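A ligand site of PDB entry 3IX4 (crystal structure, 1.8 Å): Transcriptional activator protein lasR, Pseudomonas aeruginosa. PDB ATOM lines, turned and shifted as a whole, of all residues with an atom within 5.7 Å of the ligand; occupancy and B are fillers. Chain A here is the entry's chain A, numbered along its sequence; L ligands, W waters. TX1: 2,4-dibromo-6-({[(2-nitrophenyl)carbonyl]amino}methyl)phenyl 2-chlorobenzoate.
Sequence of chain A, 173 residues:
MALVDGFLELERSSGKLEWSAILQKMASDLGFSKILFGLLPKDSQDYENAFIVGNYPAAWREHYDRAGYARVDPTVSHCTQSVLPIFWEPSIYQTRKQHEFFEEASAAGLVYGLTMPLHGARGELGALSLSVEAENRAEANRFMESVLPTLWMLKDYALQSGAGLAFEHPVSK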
ATOM      1  N   LEU A  36      -5.172  20.808 -18.234  1.00  0.00           N
ATOM      2  CA  LEU A  36      -5.134  21.922 -17.295  1.00  0.00           C
ATOM      3  C   LEU A  36      -5.581  23.197 -17.999  1.00  0.00           C
ATOM      4  O   LEU A  36      -5.040  23.587 -19.034  1.00  0.00           O
ATOM      5  CB  LEU A  36      -3.761  22.084 -16.636  1.00  0.00           C
ATOM      6  CG  LEU A  36      -3.595  23.199 -15.580  1.00  0.00           C
ATOM      7  CD1 LEU A  36      -2.598  22.817 -14.500  1.00  0.00           C
ATOM      8  CD2 LEU A  36      -3.177  24.509 -16.220  1.00  0.00           C
ATOM      9  N   PHE A  37      -6.597  23.835 -17.413  1.00  0.00           N
ATOM     10  CA  PHE A  37      -7.043  25.154 -17.810  1.00  0.00           C
ATOM     11  C   PHE A  37      -6.594  26.107 -16.695  1.00  0.00           C
ATOM     12  O   PHE A  37      -7.005  25.954 -15.543  1.00  0.00           O
ATOM     13  CB  PHE A  37      -8.575  25.147 -17.955  1.00  0.00           C
ATOM     14  CG  PHE A  37      -9.168  26.483 -18.316  1.00  0.00           C
ATOM     15  CD1 PHE A  37      -9.299  26.870 -19.642  1.00  0.00           C
ATOM     16  CD2 PHE A  37      -9.589  27.349 -17.316  1.00  0.00           C
ATOM     17  CE1 PHE A  37      -9.854  28.115 -19.973  1.00  0.00           C
ATOM     18  CE2 PHE A  37     -10.150  28.598 -17.631  1.00  0.00           C
ATOM     19  CZ  PHE A  37     -10.275  28.975 -18.965  1.00  0.00           C
ATOM     20  N   GLY A  38      -5.733  27.052 -17.040  1.00  0.00           N
ATOM     21  CA  GLY A  38      -5.189  28.018 -16.097  1.00  0.00           C
ATOM     22  C   GLY A  38      -5.432  29.429 -16.590  1.00  0.00           C
ATOM     23  O   GLY A  38      -5.248  29.722 -17.771  1.00  0.00           O
ATOM     24  N   LEU A  39      -5.855  30.313 -15.689  1.00  0.00           N
ATOM     25  CA  LEU A  39      -6.207  31.675 -16.098  1.00  0.00           C
ATOM     26  C   LEU A  39      -5.854  32.739 -15.056  1.00  0.00           C
ATOM     27  O   LEU A  39      -6.078  32.554 -13.854  1.00  0.00           O
ATOM     28  CB  LEU A  39      -7.695  31.741 -16.466  1.00  0.00           C
ATOM     29  CG  LEU A  39      -8.229  32.926 -17.281  1.00  0.00           C
ATOM     30  CD1 LEU A  39      -7.600  32.978 -18.674  1.00  0.00           C
ATOM     31  CD2 LEU A  39      -9.723  32.817 -17.380  1.00  0.00           C
ATOM     32  N   LEU A  40      -5.293  33.839 -15.550  1.00  0.00           N
ATOM     33  CA  LEU A  40      -4.944  34.989 -14.719  1.00  0.00           C
ATOM     34  C   LEU A  40      -5.734  36.216 -15.185  1.00  0.00           C
ATOM     35  O   LEU A  40      -6.045  36.353 -16.372  1.00  0.00           O
ATOM     36  CB  LEU A  40      -3.442  35.287 -14.780  1.00  0.00           C
ATOM     37  CG  LEU A  40      -2.456  34.341 -14.081  1.00  0.00           C
ATOM     38  CD1 LEU A  40      -1.034  34.632 -14.541  1.00  0.00           C
ATOM     39  CD2 LEU A  40      -2.549  34.432 -12.559  1.00  0.00           C
ATOM     40  N   TYR A  47       1.245  33.356 -11.072  1.00  0.00           N
ATOM     41  CA  TYR A  47       0.946  32.003 -11.559  1.00  0.00           C
ATOM     42  C   TYR A  47       0.614  31.031 -10.435  1.00  0.00           C
ATOM     43  O   TYR A  47      -0.213  30.129 -10.598  1.00  0.00           O
ATOM     44  CB  TYR A  47       2.102  31.463 -12.394  1.00  0.00           C
ATOM     45  CG  TYR A  47       2.328  32.238 -13.669  1.00  0.00           C
ATOM     46  CD1 TYR A  47       3.317  33.204 -13.758  1.00  0.00           C
ATOM     47  CD2 TYR A  47       1.526  32.009 -14.794  1.00  0.00           C
ATOM     48  CE1 TYR A  47       3.525  33.928 -14.931  1.00  0.00           C
ATOM     49  CE2 TYR A  47       1.720  32.728 -15.970  1.00  0.00           C
ATOM     50  CZ  TYR A  47       2.716  33.683 -16.030  1.00  0.00           C
ATOM     51  OH  TYR A  47       2.912  34.385 -17.183  1.00  0.00           O
ATOM     52  N   GLU A  48       1.265  31.239  -9.291  1.00  0.00           N
ATOM     53  CA  GLU A  48       1.050  30.424  -8.096  1.00  0.00           C
ATOM     54  C   GLU A  48      -0.352  30.613  -7.492  1.00  0.00           C
ATOM     55  O   GLU A  48      -0.770  29.836  -6.642  1.00  0.00           O
ATOM     56  CB  GLU A  48       2.152  30.710  -7.063  1.00  0.00           C
ATOM     57  CG  GLU A  48       3.527  30.090  -7.374  1.00  0.00           C
ATOM     58  CD  GLU A  48       4.334  30.833  -8.453  1.00  0.00           C
ATOM     59  OE1 GLU A  48       3.932  31.927  -8.895  1.00  0.00           O
ATOM     60  OE2 GLU A  48       5.408  30.304  -8.861  1.00  0.00           O
ATOM     61  N   ALA A  50      -3.115  31.293  -9.785  1.00  0.00           N
ATOM     62  CA  ALA A  50      -4.002  31.271 -10.962  1.00  0.00           C
ATOM     63  C   ALA A  50      -5.308  30.529 -10.683  1.00  0.00           C
ATOM     64  O   ALA A  50      -5.384  29.713  -9.762  1.00  0.00           O
ATOM     65  CB  ALA A  50      -3.277  30.642 -12.144  1.00  0.00           C
ATOM     66  N   PHE A  51      -6.332  30.833 -11.470  1.00  0.00           N
ATOM     67  CA  PHE A  51      -7.560  30.040 -11.485  1.00  0.00           C
ATOM     68  C   PHE A  51      -7.246  28.792 -12.300  1.00  0.00           C
ATOM     69  O   PHE A  51      -6.975  28.872 -13.497  1.00  0.00           O
ATOM     70  CB  PHE A  51      -8.688  30.844 -12.130  1.00  0.00           C
ATOM     71  CG  PHE A  51      -9.960  30.058 -12.348  1.00  0.00           C
ATOM     72  CD1 PHE A  51     -10.903  29.931 -11.326  1.00  0.00           C
ATOM     73  CD2 PHE A  51     -10.223  29.463 -13.572  1.00  0.00           C
ATOM     74  CE1 PHE A  51     -12.088  29.212 -11.527  1.00  0.00           C
ATOM     75  CE2 PHE A  51     -11.403  28.739 -13.789  1.00  0.00           C
ATOM     76  CZ  PHE A  51     -12.334  28.617 -12.764  1.00  0.00           C
ATOM     77  N   ILE A  52      -7.285  27.630 -11.639  1.00  0.00           N
ATOM     78  CA  ILE A  52      -6.866  26.386 -12.271  1.00  0.00           C
ATOM     79  C   ILE A  52      -7.971  25.344 -12.294  1.00  0.00           C
ATOM     80  O   ILE A  52      -8.647  25.111 -11.282  1.00  0.00           O
ATOM     81  CB  ILE A  52      -5.560  25.839 -11.624  1.00  0.00           C
ATOM     82  CG1 ILE A  52      -4.400  26.790 -11.935  1.00  0.00           C
ATOM     83  CG2 ILE A  52      -5.245  24.423 -12.113  1.00  0.00           C
ATOM     84  CD1 ILE A  52      -3.110  26.491 -11.201  1.00  0.00           C
ATOM     85  N   TYR A  56      -4.916  17.162 -13.923  1.00  0.00           N
ATOM     86  CA  TYR A  56      -3.499  16.944 -13.664  1.00  0.00           C
ATOM     87  C   TYR A  56      -3.378  16.355 -12.250  1.00  0.00           C
ATOM     88  O   TYR A  56      -4.125  16.770 -11.362  1.00  0.00           O
ATOM     89  CB  TYR A  56      -2.725  18.259 -13.714  1.00  0.00           C
ATOM     90  CG  TYR A  56      -2.198  18.687 -15.069  1.00  0.00           C
ATOM     91  CD1 TYR A  56      -1.123  19.574 -15.160  1.00  0.00           C
ATOM     92  CD2 TYR A  56      -2.751  18.214 -16.256  1.00  0.00           C
ATOM     93  CE1 TYR A  56      -0.629  19.995 -16.393  1.00  0.00           C
ATOM     94  CE2 TYR A  56      -2.255  18.623 -17.511  1.00  0.00           C
ATOM     95  CZ  TYR A  56      -1.189  19.513 -17.561  1.00  0.00           C
ATOM     96  OH  TYR A  56      -0.681  19.928 -18.775  1.00  0.00           O
ATOM     97  N   TRP A  60       1.579  16.731  -8.641  1.00  0.00           N
ATOM     98  CA  TRP A  60       2.284  17.465  -9.694  1.00  0.00           C
ATOM     99  C   TRP A  60       1.968  18.973  -9.648  1.00  0.00           C
ATOM    100  O   TRP A  60       2.874  19.806  -9.717  1.00  0.00           O
ATOM    101  CB  TRP A  60       1.970  16.887 -11.076  1.00  0.00           C
ATOM    102  CG  TRP A  60       2.478  17.736 -12.217  1.00  0.00           C
ATOM    103  CD1 TRP A  60       1.726  18.326 -13.197  1.00  0.00           C
ATOM    104  CD2 TRP A  60       3.848  18.112 -12.485  1.00  0.00           C
ATOM    105  NE1 TRP A  60       2.543  19.036 -14.050  1.00  0.00           N
ATOM    106  CE2 TRP A  60       3.841  18.933 -13.634  1.00  0.00           C
ATOM    107  CE3 TRP A  60       5.064  17.840 -11.850  1.00  0.00           C
ATOM    108  CZ2 TRP A  60       5.007  19.470 -14.179  1.00  0.00           C
ATOM    109  CZ3 TRP A  60       6.233  18.385 -12.390  1.00  0.00           C
ATOM    110  CH2 TRP A  60       6.188  19.184 -13.540  1.00  0.00           C
ATOM    111  N   ARG A  61       0.690  19.309  -9.518  1.00  0.00           N
ATOM    112  CA  ARG A  61       0.292  20.703  -9.425  1.00  0.00           C
ATOM    113  C   ARG A  61       0.959  21.401  -8.241  1.00  0.00           C
ATOM    114  O   ARG A  61       1.436  22.525  -8.362  1.00  0.00           O
ATOM    115  CB  ARG A  61      -1.228  20.845  -9.360  1.00  0.00           C
ATOM    116  CG  ARG A  61      -1.909  20.649 -10.705  1.00  0.00           C
ATOM    117  CD  ARG A  61      -3.408  20.477 -10.564  1.00  0.00           C
ATOM    118  NE  ARG A  61      -4.074  21.754 -10.277  1.00  0.00           N
ATOM    119  CZ  ARG A  61      -4.582  22.090  -9.103  1.00  0.00           C
ATOM    120  NH1 ARG A  61      -4.504  21.253  -8.071  1.00  0.00           N
ATOM    121  NH2 ARG A  61      -5.186  23.273  -8.965  1.00  0.00           N
ATOM    122  N   TYR A  64       4.722  21.767  -9.001  1.00  0.00           N
ATOM    123  CA  TYR A  64       4.837  22.878  -9.955  1.00  0.00           C
ATOM    124  C   TYR A  64       4.909  24.228  -9.242  1.00  0.00           C
ATOM    125  O   TYR A  64       5.792  25.046  -9.533  1.00  0.00           O
ATOM    126  CB  TYR A  64       3.680  22.837 -10.964  1.00  0.00           C
ATOM    127  CG  TYR A  64       3.851  23.764 -12.159  1.00  0.00           C
ATOM    128  CD1 TYR A  64       4.203  23.256 -13.413  1.00  0.00           C
ATOM    129  CD2 TYR A  64       3.622  25.132 -12.048  1.00  0.00           C
ATOM    130  CE1 TYR A  64       4.352  24.094 -14.523  1.00  0.00           C
ATOM    131  CE2 TYR A  64       3.765  25.981 -13.150  1.00  0.00           C
ATOM    132  CZ  TYR A  64       4.132  25.459 -14.377  1.00  0.00           C
ATOM    133  OH  TYR A  64       4.258  26.295 -15.449  1.00  0.00           O
ATOM    134  N   ASP A  65       3.984  24.462  -8.314  1.00  0.00           N
ATOM    135  CA  ASP A  65       3.951  25.697  -7.517  1.00  0.00           C
ATOM    136  C   ASP A  65       5.156  25.799  -6.590  1.00  0.00           C
ATOM    137  O   ASP A  65       5.806  26.849  -6.517  1.00  0.00           O
ATOM    138  CB  ASP A  65       2.665  25.751  -6.672  1.00  0.00           C
ATOM    139  CG  ASP A  65       1.454  26.199  -7.463  1.00  0.00           C
ATOM    140  OD1 ASP A  65       1.600  26.589  -8.644  1.00  0.00           O
ATOM    141  OD2 ASP A  65       0.334  26.163  -6.897  1.00  0.00           O
ATOM    142  N   ALA A  70       6.745  27.833 -13.046  1.00  0.00           N
ATOM    143  CA  ALA A  70       6.262  28.895 -13.944  1.00  0.00           C
ATOM    144  C   ALA A  70       7.412  29.730 -14.528  1.00  0.00           C
ATOM    145  O   ALA A  70       7.286  30.287 -15.616  1.00  0.00           O
ATOM    146  CB  ALA A  70       5.263  29.800 -13.210  1.00  0.00           C
ATOM    147  N   ASP A  73       9.114  26.313 -16.959  1.00  0.00           N
ATOM    148  CA  ASP A  73       8.198  25.809 -17.993  1.00  0.00           C
ATOM    149  C   ASP A  73       8.214  26.713 -19.219  1.00  0.00           C
ATOM    150  O   ASP A  73       7.761  27.850 -19.151  1.00  0.00           O
ATOM    151  CB  ASP A  73       6.793  25.743 -17.379  1.00  0.00           C
ATOM    152  CG  ASP A  73       5.721  25.270 -18.354  1.00  0.00           C
ATOM    153  OD1 ASP A  73       5.981  25.091 -19.567  1.00  0.00           O
ATOM    154  OD2 ASP A  73       4.582  25.097 -17.876  1.00  0.00           O
ATOM    155  N   THR A  75       6.437  26.762 -21.865  1.00  0.00           N
ATOM    156  CA  THR A  75       5.129  27.128 -22.423  1.00  0.00           C
ATOM    157  C   THR A  75       4.613  28.434 -21.813  1.00  0.00           C
ATOM    158  O   THR A  75       3.825  29.140 -22.454  1.00  0.00           O
ATOM    159  CB  THR A  75       4.080  26.003 -22.274  1.00  0.00           C
ATOM    160  OG1 THR A  75       3.740  25.834 -20.888  1.00  0.00           O
ATOM    161  CG2 THR A  75       4.601  24.687 -22.854  1.00  0.00           C
ATOM    162  N   VAL A  76       5.056  28.758 -20.604  1.00  0.00           N
ATOM    163  CA  VAL A  76       4.604  29.971 -19.905  1.00  0.00           C
ATOM    164  C   VAL A  76       5.032  31.236 -20.655  1.00  0.00           C
ATOM    165  O   VAL A  76       4.192  32.059 -21.018  1.00  0.00           O
ATOM    166  CB  VAL A  76       5.066  30.012 -18.421  1.00  0.00           C
ATOM    167  CG1 VAL A  76       4.709  31.343 -17.766  1.00  0.00           C
ATOM    168  CG2 VAL A  76       4.450  28.854 -17.641  1.00  0.00           C
ATOM    169  N   CYS A  79       3.318  31.643 -23.975  1.00  0.00           N
ATOM    170  CA  CYS A  79       1.960  32.165 -23.851  1.00  0.00           C
ATOM    171  C   CYS A  79       1.912  33.690 -23.748  1.00  0.00           C
ATOM    172  O   CYS A  79       0.974  34.314 -24.228  1.00  0.00           O
ATOM    173  CB  CYS A  79       1.223  31.511 -22.687  1.00  0.00           C
ATOM    174  SG  CYS A  79       0.743  29.790 -22.997  1.00  0.00           S
ATOM    175  N   TRP A  88       4.617  20.146 -27.137  1.00  0.00           N
ATOM    176  CA  TRP A  88       5.609  19.700 -26.167  1.00  0.00           C
ATOM    177  C   TRP A  88       6.715  18.917 -26.867  1.00  0.00           C
ATOM    178  O   TRP A  88       6.916  17.719 -26.625  1.00  0.00           O
ATOM    179  CB  TRP A  88       4.973  18.881 -25.057  1.00  0.00           C
ATOM    180  CG  TRP A  88       3.856  19.591 -24.286  1.00  0.00           C
ATOM    181  CD1 TRP A  88       3.463  20.888 -24.428  1.00  0.00           C
ATOM    182  CD2 TRP A  88       3.039  19.024 -23.263  1.00  0.00           C
ATOM    183  NE1 TRP A  88       2.417  21.161 -23.550  1.00  0.00           N
ATOM    184  CE2 TRP A  88       2.149  20.034 -22.822  1.00  0.00           C
ATOM    185  CE3 TRP A  88       2.964  17.755 -22.667  1.00  0.00           C
ATOM    186  CZ2 TRP A  88       1.198  19.817 -21.816  1.00  0.00           C
ATOM    187  CZ3 TRP A  88       2.022  17.536 -21.663  1.00  0.00           C
ATOM    188  CH2 TRP A  88       1.152  18.566 -21.246  1.00  0.00           C
ATOM    189  N   ILE A  92      11.772  22.428 -27.213  1.00  0.00           N
ATOM    190  CA  ILE A  92      11.359  23.508 -26.317  1.00  0.00           C
ATOM    191  C   ILE A  92      12.036  23.460 -24.940  1.00  0.00           C
ATOM    192  O   ILE A  92      12.049  24.458 -24.210  1.00  0.00           O
ATOM    193  CB  ILE A  92       9.805  23.667 -26.199  1.00  0.00           C
ATOM    194  CG1 ILE A  92       9.184  22.575 -25.306  1.00  0.00           C
ATOM    195  CG2 ILE A  92       9.163  23.729 -27.580  1.00  0.00           C
ATOM    196  CD1 ILE A  92       7.732  22.862 -24.864  1.00  0.00           C
ATOM    197  N   TYR A  93      12.608  22.308 -24.602  1.00  0.00           N
ATOM    198  CA  TYR A  93      13.300  22.141 -23.328  1.00  0.00           C
ATOM    199  C   TYR A  93      14.797  22.338 -23.576  1.00  0.00           C
ATOM    200  O   TYR A  93      15.506  21.412 -23.979  1.00  0.00           O
ATOM    201  CB  TYR A  93      12.997  20.770 -22.716  1.00  0.00           C
ATOM    202  CG  TYR A  93      11.506  20.495 -22.639  1.00  0.00           C
ATOM    203  CD1 TYR A  93      10.884  19.660 -23.566  1.00  0.00           C
ATOM    204  CD2 TYR A  93      10.729  21.085 -21.644  1.00  0.00           C
ATOM    205  CE1 TYR A  93       9.494  19.406 -23.493  1.00  0.00           C
ATOM    206  CE2 TYR A  93       9.356  20.843 -21.563  1.00  0.00           C
ATOM    207  CZ  TYR A  93       8.755  20.011 -22.489  1.00  0.00           C
ATOM    208  OH  TYR A  93       7.399  19.776 -22.392  1.00  0.00           O
ATOM    209  N   PHE A 101      12.504  19.769 -15.645  1.00  0.00           N
ATOM    210  CA  PHE A 101      11.065  20.010 -15.736  1.00  0.00           C
ATOM    211  C   PHE A 101      10.404  18.943 -16.608  1.00  0.00           C
ATOM    212  O   PHE A 101       9.389  18.371 -16.225  1.00  0.00           O
ATOM    213  CB  PHE A 101      10.769  21.407 -16.286  1.00  0.00           C
ATOM    214  CG  PHE A 101       9.308  21.626 -16.592  1.00  0.00           C
ATOM    215  CD1 PHE A 101       8.402  21.874 -15.568  1.00  0.00           C
ATOM    216  CD2 PHE A 101       8.842  21.553 -17.900  1.00  0.00           C
ATOM    217  CE1 PHE A 101       7.052  22.063 -15.830  1.00  0.00           C
ATOM    218  CE2 PHE A 101       7.493  21.730 -18.183  1.00  0.00           C
ATOM    219  CZ  PHE A 101       6.595  21.993 -17.148  1.00  0.00           C
ATOM    220  N   ALA A 105       7.692  16.305 -15.156  1.00  0.00           N
ATOM    221  CA  ALA A 105       6.366  16.236 -15.774  1.00  0.00           C
ATOM    222  C   ALA A 105       6.094  14.857 -16.370  1.00  0.00           C
ATOM    223  O   ALA A 105       4.986  14.335 -16.254  1.00  0.00           O
ATOM    224  CB  ALA A 105       6.207  17.320 -16.842  1.00  0.00           C
ATOM    225  N   LEU A 110       2.954  13.187 -17.900  1.00  0.00           N
ATOM    226  CA  LEU A 110       2.692  14.286 -18.811  1.00  0.00           C
ATOM    227  C   LEU A 110       3.908  14.502 -19.712  1.00  0.00           C
ATOM    228  O   LEU A 110       4.779  15.322 -19.426  1.00  0.00           O
ATOM    229  CB  LEU A 110       2.348  15.561 -18.012  1.00  0.00           C
ATOM    230  CG  LEU A 110       1.118  15.433 -17.095  1.00  0.00           C
ATOM    231  CD1 LEU A 110       1.136  16.453 -15.974  1.00  0.00           C
ATOM    232  CD2 LEU A 110      -0.173  15.551 -17.888  1.00  0.00           C
ATOM    233  N   THR A 115       0.224  23.138 -25.492  1.00  0.00           N
ATOM    234  CA  THR A 115      -0.362  24.205 -24.705  1.00  0.00           C
ATOM    235  C   THR A 115      -0.895  25.273 -25.633  1.00  0.00           C
ATOM    236  O   THR A 115      -0.173  25.796 -26.493  1.00  0.00           O
ATOM    237  CB  THR A 115       0.680  24.790 -23.720  1.00  0.00           C
ATOM    238  OG1 THR A 115       1.073  23.761 -22.791  1.00  0.00           O
ATOM    239  CG2 THR A 115       0.117  25.978 -22.969  1.00  0.00           C
ATOM    240  N   LEU A 125      -5.101  36.278 -19.143  1.00  0.00           N
ATOM    241  CA  LEU A 125      -3.950  35.551 -19.655  1.00  0.00           C
ATOM    242  C   LEU A 125      -4.004  34.135 -19.107  1.00  0.00           C
ATOM    243  O   LEU A 125      -4.042  33.942 -17.887  1.00  0.00           O
ATOM    244  CB  LEU A 125      -2.634  36.242 -19.260  1.00  0.00           C
ATOM    245  CG  LEU A 125      -1.293  35.515 -19.436  1.00  0.00           C
ATOM    246  CD1 LEU A 125      -0.922  35.380 -20.912  1.00  0.00           C
ATOM    247  CD2 LEU A 125      -0.177  36.227 -18.661  1.00  0.00           C
ATOM    248  N   GLY A 126      -4.025  33.152 -20.001  1.00  0.00           N
ATOM    249  CA  GLY A 126      -4.192  31.760 -19.577  1.00  0.00           C
ATOM    250  C   GLY A 126      -3.554  30.762 -20.516  1.00  0.00           C
ATOM    251  O   GLY A 126      -2.844  31.120 -21.449  1.00  0.00           O
ATOM    252  N   ALA A 127      -3.817  29.486 -20.248  1.00  0.00           N
ATOM    253  CA  ALA A 127      -3.333  28.410 -21.085  1.00  0.00           C
ATOM    254  C   ALA A 127      -4.290  27.228 -20.972  1.00  0.00           C
ATOM    255  O   ALA A 127      -4.750  26.913 -19.875  1.00  0.00           O
ATOM    256  CB  ALA A 127      -1.967  27.985 -20.650  1.00  0.00           C
ATOM    257  N   SER A 129      -3.749  23.433 -21.552  1.00  0.00           N
ATOM    258  CA  SER A 129      -2.771  22.389 -21.837  1.00  0.00           C
ATOM    259  C   SER A 129      -3.485  21.067 -21.872  1.00  0.00           C
ATOM    260  O   SER A 129      -4.356  20.795 -21.025  1.00  0.00           O
ATOM    261  CB  SER A 129      -1.667  22.378 -20.776  1.00  0.00           C
ATOM    262  OG  SER A 129      -0.922  23.589 -20.790  1.00  0.00           O
HETATM  263  C1  TX1 L   1       0.671  26.182 -15.550  1.00  0.00           C
HETATM  264  C2  TX1 L   1       0.450  26.179 -14.088  1.00  0.00           C
HETATM  265  C3  TX1 L   1       0.502  24.972 -13.404  1.00  0.00           C
HETATM  266  C4  TX1 L   1       0.784  23.798 -14.100  1.00  0.00           C
HETATM  267  C5  TX1 L   1       0.991  23.753 -15.484  1.00  0.00           C
HETATM  268  C6  TX1 L   1       0.959  24.911 -16.243  1.00  0.00           C
HETATM  269  C7  TX1 L   1       1.180  24.915 -17.742  1.00  0.00           C
HETATM  270  N8  TX1 L   1       2.163  23.905 -18.116  1.00  0.00           N
HETATM  271  C9  TX1 L   1       1.838  22.697 -18.567  1.00  0.00           C
HETATM  272  C10 TX1 L   1       2.900  21.860 -19.217  1.00  0.00           C
HETATM  273  C11 TX1 L   1       3.441  22.269 -20.425  1.00  0.00           C
HETATM  274  C12 TX1 L   1       4.432  21.491 -21.038  1.00  0.00           C
HETATM  275  C13 TX1 L   1       4.887  20.313 -20.475  1.00  0.00           C
HETATM  276  C14 TX1 L   1       4.366  19.855 -19.267  1.00  0.00           C
HETATM  277  C15 TX1 L   1       3.384  20.581 -18.606  1.00  0.00           C
HETATM  278  N16 TX1 L   1       2.879  20.131 -17.381  1.00  0.00           N
HETATM  279  O17 TX1 L   1       0.708  22.248 -18.446  1.00  0.00           O
HETATM  280  O18 TX1 L   1       2.835  18.942 -17.102  1.00  0.00           O
HETATM  281  O19 TX1 L   1       2.482  21.068 -16.442  1.00  0.00           O
HETATM  282  O20 TX1 L   1       0.630  27.369 -16.212  1.00  0.00           O
HETATM  283  C21 TX1 L   1      -0.619  28.019 -16.525  1.00  0.00           C
HETATM  284  O22 TX1 L   1      -1.679  27.523 -16.181  1.00  0.00           O
HETATM  285 BR23 TX1 L   1       0.105  27.818 -13.229  1.00  0.00          BR
HETATM  286 BR24 TX1 L   1       0.850  22.194 -13.126  1.00  0.00          BR
HETATM  287  C25 TX1 L   1      -0.513  29.312 -17.268  1.00  0.00           C
HETATM  288  C26 TX1 L   1       0.380  29.413 -18.331  1.00  0.00           C
HETATM  289  C27 TX1 L   1       0.492  30.604 -19.026  1.00  0.00           C
HETATM  290  C28 TX1 L   1      -0.261  31.723 -18.663  1.00  0.00           C
HETATM  291  C29 TX1 L   1      -1.147  31.680 -17.594  1.00  0.00           C
HETATM  292  C30 TX1 L   1      -1.302  30.504 -16.873  1.00  0.00           C
HETATM  293 CL31 TX1 L   1      -2.441  30.437 -15.492  1.00  0.00          CL
HETATM  294  O   HOH W   1       2.110  33.341 -19.564  1.00  0.00           O
HETATM  295  O   HOH W   2       1.842  27.602 -20.184  1.00  0.00           O
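NE1 of Trp 88 sits at hydrogen-bond distance from OG1 of Thr 115, at 3.0 Å.
The backbone carbonyl oxygen (O) of Thr 75 sits at hydrogen-bond distance from the side-chain sulfur (SG) of Cys 79, at 3.2 Å.
The backbone NH (N) of Ala 127 sits at hydrogen-bond distance from the backbone carbonyl oxygen (O) of Gly 38 (2.9 Å).
O of Phe 51 lies within hydrogen-bond range of N of Leu 39, at 2.9 Å.
The side-chain hydroxyl (OG1) of Thr 115 sits at hydrogen-bond distance from the side-chain hydroxyl (OG) of Ser 129 (2.8 Å).
OD1 of Asp 73 lies within hydrogen-bond range of OG1 of Thr 75 (2.7 Å).
The backbone NH (N) of Ser 129 is in hydrogen-bond range of the backbone carbonyl oxygen (O) of Leu 36, at 2.8 Å.
O of Leu 125 is in hydrogen-bond range of N of Leu 40, 2.7 Å away.
O17 of the ligand sits at hydrogen-bond distance from OH of Tyr 56, at 2.7 Å.
An oxygen (O17) of the ligand lies within hydrogen-bond range of the side-chain hydroxyl (OG) of Ser 129 (3.2 Å).
OD2 of Asp 73 is in hydrogen-bond range of N8 of the ligand (2.7 Å).
An oxygen (O18) of the ligand lies within hydrogen-bond range of the indole nitrogen of Trp 60 (3.1 Å).
CD2 of Leu 36 touches O22 of the ligand, 3.4 Å away.
C of Gly 38 touches CL31 of the ligand (3.3 Å).
Leu 39 touches the ligand.
Tyr 47 touches the ligand (CE2 to C29, 3.5 Å).
CB of Ala 50 touches CL31 of the ligand, at 3.5 Å.
Arg 61 touches the ligand.
CD2 of Tyr 64 touches C3 of the ligand (3.4 Å).
Thr 75 touches the ligand (OG1 to C11, 3.6 Å).
Cys 79 touches the ligand.
Trp 88 touches the ligand.
Tyr 93 touches the ligand (OH to C13, 3.2 Å).
CZ of Phe 101 touches C14 of the ligand, at 3.7 Å.
Ala 105 touches the ligand (CB to O18, 3.8 Å).
Leu 110 touches the ligand (CD1 to O18, 3.2 Å).
Thr 115 touches the ligand.
Leu 125 touches the ligand.
Gly 126 touches the ligand (CA to C29, 3.6 Å).
CB of Ala 127 touches C26 of the ligand, 3.6 Å away.
Hydrophobic or aromatic side chains that line the ligand: Leu 36, Tyr 47, Ala 50, Tyr 56, Trp 60, Tyr 64, Trp 88, Phe 101, Ala 105, Leu 110 and Ala 127.
Along chain A the residues within 4 Å of the ligand span positions 36 to 129.
The nearest printed residue that does not touch the ligand is Ile 52 (4.03 Å).
Water W2 lies within hydrogen-bond range of the side-chain hydroxyl of Thr 75 (2.7 Å), the backbone NH of Val 76 (3.4 Å) and the side-chain sulfur of Cys 79 (3.7 Å).
Water W1 bridges the side-chain hydroxyl (OH) of Tyr 47 (2.7 Å) and the backbone carbonyl oxygen (O) of Val 76 (2.8 Å).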
